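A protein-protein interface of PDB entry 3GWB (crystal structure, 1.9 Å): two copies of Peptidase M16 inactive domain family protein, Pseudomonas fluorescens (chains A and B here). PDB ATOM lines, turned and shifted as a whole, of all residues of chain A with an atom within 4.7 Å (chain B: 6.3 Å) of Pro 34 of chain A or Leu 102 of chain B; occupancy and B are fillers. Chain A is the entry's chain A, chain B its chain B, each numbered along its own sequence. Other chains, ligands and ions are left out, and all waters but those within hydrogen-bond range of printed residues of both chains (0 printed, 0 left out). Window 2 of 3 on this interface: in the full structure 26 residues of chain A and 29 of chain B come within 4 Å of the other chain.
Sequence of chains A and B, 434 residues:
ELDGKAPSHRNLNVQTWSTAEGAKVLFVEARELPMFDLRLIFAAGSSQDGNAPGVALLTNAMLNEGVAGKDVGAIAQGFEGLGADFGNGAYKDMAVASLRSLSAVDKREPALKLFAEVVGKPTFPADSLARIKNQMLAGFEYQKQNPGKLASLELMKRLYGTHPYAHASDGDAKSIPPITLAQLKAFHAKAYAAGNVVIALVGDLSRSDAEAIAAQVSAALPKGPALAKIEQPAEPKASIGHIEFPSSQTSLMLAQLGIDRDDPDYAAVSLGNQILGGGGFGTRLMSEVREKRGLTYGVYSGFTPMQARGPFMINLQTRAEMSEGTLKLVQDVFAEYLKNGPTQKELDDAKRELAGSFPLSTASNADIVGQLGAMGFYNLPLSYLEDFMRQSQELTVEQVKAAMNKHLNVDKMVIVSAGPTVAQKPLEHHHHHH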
ATOM      1  N   GLU A  32      -2.101  24.022   7.909  1.00  0.00           N
ATOM      2  CA  GLU A  32      -2.506  25.153   7.068  1.00  0.00           C
ATOM      3  C   GLU A  32      -3.050  24.770   5.691  1.00  0.00           C
ATOM      4  O   GLU A  32      -4.069  25.302   5.249  1.00  0.00           O
ATOM      5  CB  GLU A  32      -1.344  26.138   6.902  1.00  0.00           C
ATOM      6  CG  GLU A  32      -0.010  25.508   6.492  1.00  0.00           C
ATOM      7  CD  GLU A  32       0.797  24.965   7.674  1.00  0.00           C
ATOM      8  OE1 GLU A  32       1.956  24.545   7.452  1.00  0.00           O
ATOM      9  OE2 GLU A  32       0.287  24.961   8.815  1.00  0.00           O
ATOM     10  N   LEU A  33      -2.371  23.848   5.016  1.00  0.00           N
ATOM     11  CA  LEU A  33      -2.775  23.398   3.681  1.00  0.00           C
ATOM     12  C   LEU A  33      -3.191  21.932   3.688  1.00  0.00           C
ATOM     13  O   LEU A  33      -2.614  21.120   4.415  1.00  0.00           O
ATOM     14  CB  LEU A  33      -1.615  23.581   2.699  1.00  0.00           C
ATOM     15  CG  LEU A  33      -1.121  25.020   2.560  1.00  0.00           C
ATOM     16  CD1 LEU A  33       0.253  25.040   1.896  1.00  0.00           C
ATOM     17  CD2 LEU A  33      -2.140  25.824   1.764  1.00  0.00           C
ATOM     18  N   PRO A  34      -4.186  21.572   2.857  1.00  0.00           N
ATOM     19  CA  PRO A  34      -4.700  20.202   2.749  1.00  0.00           C
ATOM     20  C   PRO A  34      -3.787  19.294   1.925  1.00  0.00           C
ATOM     21  O   PRO A  34      -4.206  18.681   0.941  1.00  0.00           O
ATOM     22  CB  PRO A  34      -6.060  20.410   2.095  1.00  0.00           C
ATOM     23  CG  PRO A  34      -5.762  21.519   1.118  1.00  0.00           C
ATOM     24  CD  PRO A  34      -4.937  22.483   1.968  1.00  0.00           C
ATOM     25  N   MET A  35      -2.533  19.206   2.335  1.00  0.00           N
ATOM     26  CA  MET A  35      -1.566  18.385   1.623  1.00  0.00           C
ATOM     27  C   MET A  35      -0.406  18.042   2.532  1.00  0.00           C
ATOM     28  O   MET A  35      -0.323  18.533   3.653  1.00  0.00           O
ATOM     29  CB  MET A  35      -1.060  19.122   0.378  1.00  0.00           C
ATOM     30  CG  MET A  35      -0.737  20.595   0.586  1.00  0.00           C
ATOM     31  SD  MET A  35      -0.421  21.495  -0.983  1.00  0.00           S
ATOM     32  CE  MET A  35      -1.533  20.612  -2.113  1.00  0.00           C
ATOM     33  N   SER A 101       1.454  15.061  -1.882  1.00  0.00           N
ATOM     34  CA  SER A 101       0.102  14.601  -2.165  1.00  0.00           C
ATOM     35  C   SER A 101      -0.973  15.350  -1.390  1.00  0.00           C
ATOM     36  O   SER A 101      -0.712  15.901  -0.318  1.00  0.00           O
ATOM     37  CB  SER A 101       0.020  13.100  -1.841  1.00  0.00           C
ATOM     38  OG  SER A 101      -1.311  12.614  -1.800  1.00  0.00           O
ATOM     39  N   LEU A 102      -2.178  15.388  -1.952  1.00  0.00           N
ATOM     40  CA  LEU A 102      -3.295  16.013  -1.272  1.00  0.00           C
ATOM     41  C   LEU A 102      -3.481  15.120  -0.046  1.00  0.00           C
ATOM     42  O   LEU A 102      -3.204  13.919  -0.110  1.00  0.00           O
ATOM     43  CB  LEU A 102      -4.545  15.975  -2.152  1.00  0.00           C
ATOM     44  CG  LEU A 102      -4.534  16.939  -3.343  1.00  0.00           C
ATOM     45  CD1 LEU A 102      -5.726  16.670  -4.245  1.00  0.00           C
ATOM     46  CD2 LEU A 102      -4.571  18.374  -2.830  1.00  0.00           C
ATOM     47  N   SER A 103      -3.946  15.699   1.058  1.00  0.00           N
ATOM     48  CA  SER A 103      -4.124  14.947   2.296  1.00  0.00           C
ATOM     49  C   SER A 103      -5.419  14.142   2.388  1.00  0.00           C
ATOM     50  O   SER A 103      -5.509  13.210   3.189  1.00  0.00           O
ATOM     51  CB  SER A 103      -4.015  15.891   3.502  1.00  0.00           C
ATOM     52  OG  SER A 103      -5.022  16.887   3.478  1.00  0.00           O
ATOM     53  N   ASP A 204      -0.647  18.115   6.536  1.00  0.00           N
ATOM     54  CA  ASP A 204      -1.977  18.007   7.110  1.00  0.00           C
ATOM     55  C   ASP A 204      -2.299  16.577   7.532  1.00  0.00           C
ATOM     56  O   ASP A 204      -3.153  15.915   6.944  1.00  0.00           O
ATOM     57  CB  ASP A 204      -2.997  18.520   6.085  1.00  0.00           C
ATOM     58  CG  ASP A 204      -4.410  18.520   6.615  1.00  0.00           C
ATOM     59  OD1 ASP A 204      -4.584  18.750   7.832  1.00  0.00           O
ATOM     60  OD2 ASP A 204      -5.344  18.305   5.809  1.00  0.00           O
ATOM     61  N   PRO B  34      -9.486  18.708  -6.583  1.00  0.00           N
ATOM     62  CA  PRO B  34      -9.840  19.994  -5.980  1.00  0.00           C
ATOM     63  C   PRO B  34      -8.794  21.066  -6.281  1.00  0.00           C
ATOM     64  O   PRO B  34      -8.270  21.703  -5.368  1.00  0.00           O
ATOM     65  CB  PRO B  34      -9.923  19.655  -4.495  1.00  0.00           C
ATOM     66  CG  PRO B  34      -8.816  18.650  -4.337  1.00  0.00           C
ATOM     67  CD  PRO B  34      -9.012  17.755  -5.559  1.00  0.00           C
ATOM     68  N   MET B  35      -8.502  21.261  -7.565  1.00  0.00           N
ATOM     69  CA  MET B  35      -7.503  22.234  -7.997  1.00  0.00           C
ATOM     70  C   MET B  35      -7.884  22.751  -9.380  1.00  0.00           C
ATOM     71  O   MET B  35      -8.824  22.252 -10.008  1.00  0.00           O
ATOM     72  CB  MET B  35      -6.120  21.580  -8.130  1.00  0.00           C
ATOM     73  CG  MET B  35      -5.712  20.588  -7.040  1.00  0.00           C
ATOM     74  SD  MET B  35      -4.154  19.727  -7.481  1.00  0.00           S
ATOM     75  CE  MET B  35      -4.471  19.296  -9.130  1.00  0.00           C
ATOM     76  N   PHE B  36      -7.132  23.742  -9.853  1.00  0.00           N
ATOM     77  CA  PHE B  36      -7.340  24.294 -11.182  1.00  0.00           C
ATOM     78  C   PHE B  36      -6.062  24.934 -11.708  1.00  0.00           C
ATOM     79  O   PHE B  36      -5.153  25.285 -10.941  1.00  0.00           O
ATOM     80  CB  PHE B  36      -8.497  25.307 -11.190  1.00  0.00           C
ATOM     81  CG  PHE B  36      -8.180  26.622 -10.536  1.00  0.00           C
ATOM     82  CD1 PHE B  36      -7.545  27.634 -11.250  1.00  0.00           C
ATOM     83  CD2 PHE B  36      -8.541  26.858  -9.217  1.00  0.00           C
ATOM     84  CE1 PHE B  36      -7.288  28.868 -10.662  1.00  0.00           C
ATOM     85  CE2 PHE B  36      -8.290  28.084  -8.621  1.00  0.00           C
ATOM     86  CZ  PHE B  36      -7.658  29.091  -9.340  1.00  0.00           C
ATOM     87  N   LEU B  82      -0.066  29.434   0.165  1.00  0.00           N
ATOM     88  CA  LEU B  82      -1.452  29.226  -0.245  1.00  0.00           C
ATOM     89  C   LEU B  82      -1.618  27.921  -1.016  1.00  0.00           C
ATOM     90  O   LEU B  82      -2.724  27.576  -1.438  1.00  0.00           O
ATOM     91  CB  LEU B  82      -1.930  30.403  -1.109  1.00  0.00           C
ATOM     92  CG  LEU B  82      -2.040  31.766  -0.418  1.00  0.00           C
ATOM     93  CD1 LEU B  82      -2.319  32.855  -1.440  1.00  0.00           C
ATOM     94  CD2 LEU B  82      -3.154  31.718   0.620  1.00  0.00           C
ATOM     95  N   GLY B  83      -0.515  27.196  -1.189  1.00  0.00           N
ATOM     96  CA  GLY B  83      -0.549  25.935  -1.908  1.00  0.00           C
ATOM     97  C   GLY B  83      -0.548  26.124  -3.415  1.00  0.00           C
ATOM     98  O   GLY B  83      -0.862  25.195  -4.162  1.00  0.00           O
ATOM     99  N   ALA B  84      -0.182  27.323  -3.858  1.00  0.00           N
ATOM    100  CA  ALA B  84      -0.166  27.646  -5.279  1.00  0.00           C
ATOM    101  C   ALA B  84       1.225  27.610  -5.897  1.00  0.00           C
ATOM    102  O   ALA B  84       2.230  27.759  -5.203  1.00  0.00           O
ATOM    103  CB  ALA B  84      -0.790  29.017  -5.498  1.00  0.00           C
ATOM    104  N   ARG B 100      -1.282  27.551 -10.639  1.00  0.00           N
ATOM    105  CA  ARG B 100      -1.926  26.290 -10.350  1.00  0.00           C
ATOM    106  C   ARG B 100      -2.272  26.502  -8.883  1.00  0.00           C
ATOM    107  O   ARG B 100      -1.445  26.974  -8.111  1.00  0.00           O
ATOM    108  CB  ARG B 100      -0.964  25.118 -10.518  1.00  0.00           C
ATOM    109  CG  ARG B 100      -1.626  23.790 -10.236  1.00  0.00           C
ATOM    110  CD  ARG B 100      -0.597  22.746  -9.872  1.00  0.00           C
ATOM    111  NE  ARG B 100      -1.209  21.618  -9.182  1.00  0.00           N
ATOM    112  CZ  ARG B 100      -0.532  20.735  -8.458  1.00  0.00           C
ATOM    113  NH1 ARG B 100       0.785  20.850  -8.330  1.00  0.00           N
ATOM    114  NH2 ARG B 100      -1.170  19.738  -7.856  1.00  0.00           N
ATOM    115  N   SER B 101      -3.498  26.185  -8.497  1.00  0.00           N
ATOM    116  CA  SER B 101      -3.902  26.413  -7.122  1.00  0.00           C
ATOM    117  C   SER B 101      -5.018  25.485  -6.662  1.00  0.00           C
ATOM    118  O   SER B 101      -5.657  24.814  -7.469  1.00  0.00           O
ATOM    119  CB  SER B 101      -4.327  27.883  -6.983  1.00  0.00           C
ATOM    120  OG  SER B 101      -5.373  28.073  -6.052  1.00  0.00           O
ATOM    121  N   LEU B 102      -5.221  25.428  -5.351  1.00  0.00           N
ATOM    122  CA  LEU B 102      -6.295  24.625  -4.790  1.00  0.00           C
ATOM    123  C   LEU B 102      -7.562  25.363  -5.212  1.00  0.00           C
ATOM    124  O   LEU B 102      -7.540  26.590  -5.361  1.00  0.00           O
ATOM    125  CB  LEU B 102      -6.180  24.596  -3.262  1.00  0.00           C
ATOM    126  CG  LEU B 102      -4.945  23.872  -2.718  1.00  0.00           C
ATOM    127  CD1 LEU B 102      -4.751  24.180  -1.232  1.00  0.00           C
ATOM    128  CD2 LEU B 102      -5.119  22.375  -2.939  1.00  0.00           C
ATOM    129  N   SER B 103      -8.652  24.625  -5.416  1.00  0.00           N
ATOM    130  CA  SER B 103      -9.926  25.212  -5.818  1.00  0.00           C
ATOM    131  C   SER B 103     -10.708  25.815  -4.640  1.00  0.00           C
ATOM    132  O   SER B 103     -11.560  26.677  -4.833  1.00  0.00           O
ATOM    133  CB  SER B 103     -10.783  24.151  -6.523  1.00  0.00           C
ATOM    134  OG  SER B 103     -10.977  23.014  -5.691  1.00  0.00           O
ATOM    135  N   ALA B 104     -10.421  25.352  -3.425  1.00  0.00           N
ATOM    136  CA  ALA B 104     -11.095  25.868  -2.236  1.00  0.00           C
ATOM    137  C   ALA B 104     -11.122  27.400  -2.280  1.00  0.00           C
ATOM    138  O   ALA B 104     -10.088  28.040  -2.469  1.00  0.00           O
ATOM    139  CB  ALA B 104     -10.372  25.392  -0.984  1.00  0.00           C
ATOM    140  N   VAL B 105     -12.306  27.979  -2.112  1.00  0.00           N
ATOM    141  CA  VAL B 105     -12.465  29.435  -2.150  1.00  0.00           C
ATOM    142  C   VAL B 105     -11.487  30.193  -1.249  1.00  0.00           C
ATOM    143  O   VAL B 105     -10.881  31.186  -1.665  1.00  0.00           O
ATOM    144  CB  VAL B 105     -13.915  29.842  -1.773  1.00  0.00           C
ATOM    145  CG1 VAL B 105     -14.318  29.191  -0.457  1.00  0.00           C
ATOM    146  CG2 VAL B 105     -14.023  31.355  -1.665  1.00  0.00           C
ATOM    147  N   LYS B 107      -8.615  29.493  -0.429  1.00  0.00           N
ATOM    148  CA  LYS B 107      -7.234  29.419  -0.888  1.00  0.00           C
ATOM    149  C   LYS B 107      -7.046  30.125  -2.222  1.00  0.00           C
ATOM    150  O   LYS B 107      -6.091  30.876  -2.408  1.00  0.00           O
ATOM    151  CB  LYS B 107      -6.788  27.961  -1.024  1.00  0.00           C
ATOM    152  CG  LYS B 107      -6.884  27.164   0.262  1.00  0.00           C
ATOM    153  CD  LYS B 107      -6.089  27.816   1.386  1.00  0.00           C
ATOM    154  CE  LYS B 107      -6.144  26.968   2.649  1.00  0.00           C
ATOM    155  NZ  LYS B 107      -5.424  27.613   3.777  1.00  0.00           N
ATOM    156  N   ARG B 108      -7.962  29.892  -3.150  1.00  0.00           N
ATOM    157  CA  ARG B 108      -7.833  30.503  -4.463  1.00  0.00           C
ATOM    158  C   ARG B 108      -8.005  32.017  -4.460  1.00  0.00           C
ATOM    159  O   ARG B 108      -7.342  32.713  -5.227  1.00  0.00           O
ATOM    160  CB  ARG B 108      -8.828  29.875  -5.436  1.00  0.00           C
ATOM    161  CG  ARG B 108     -10.240  30.396  -5.315  1.00  0.00           C
ATOM    162  CD  ARG B 108     -11.120  29.642  -6.272  1.00  0.00           C
ATOM    163  NE  ARG B 108     -12.439  30.236  -6.409  1.00  0.00           N
ATOM    164  CZ  ARG B 108     -13.551  29.524  -6.526  1.00  0.00           C
ATOM    165  NH1 ARG B 108     -13.485  28.199  -6.515  1.00  0.00           N
ATOM    166  NH2 ARG B 108     -14.720  30.130  -6.664  1.00  0.00           N
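The side-chain amino group of Lys 107 of chain B is in hydrogen-bond range of the backbone carbonyl oxygen of Glu 32 of chain A (3.1 Å).
O of Pro 34 of chain A sits at hydrogen-bond distance from N of Ser 103 of chain A, 3.0 Å away. O of Pro 34 of chain B is in hydrogen-bond range of N of Ser 103 of chain B (2.9 Å).
Leu 82 of chain B touches Leu 33 of chain A. Leu 33 of chain A touches Gly 83 of chain B (CD2 to N, 3.6 Å). CD of Pro 34 of chain A touches CD1 of Leu 102 of chain B, 3.6 Å away. Leu 102 of chain A touches Pro 34 of chain B (CD1 to CG, 3.7 Å).
Pro 34 of chain A touches just one residue of chain B: Leu 102. Leu 102 of chain B touches one residue of chain A. Printed residues of chain B within 4 Å of Leu 102 of chain A: Pro 34. Printed residues of chain A within 4 Å of Leu 82 of chain B: Leu 33 (3.5 Å). Met 35 of chain A touches none of the printed residues of chain B. Met 35 of chain B touches none of the printed residues of chain A. The nearest residue of chain A that does not touch Leu 102 of chain B is Leu 102 of chain A (4.04 Å). The nearest printed residue of chain B that does not touch Leu 102 of chain A is Leu 102 of chain B (4.04 Å).
Of the 8 printed residues of chain A, 4 touch a printed residue of chain B. Printed residues of chain A that touch a printed residue of chain B: Glu 32, Leu 33, Pro 34 and Leu 102. Hydrophobic or aromatic side chains of chain A within 4 Å of the printed part of chain B: Leu 33, Pro 34 and Leu 102. Among the printed residues, 5 pairs touch across the chains. Among the printed residues, no Asp or Glu carboxylate lies within 4 Å of a Lys or Arg side-chain nitrogen of the other chain.
Pro 34 of chain A touches Leu 102 of chain B, and with the chains exchanged Leu 102 of chain A touches Pro 34 of chain B. Positions printed for both chains: 34, 35, 101, 102 and 103. Of the 5 pairs that touch across the chains among the printed residues, 2 have their exchanged pair printed and touching as well.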
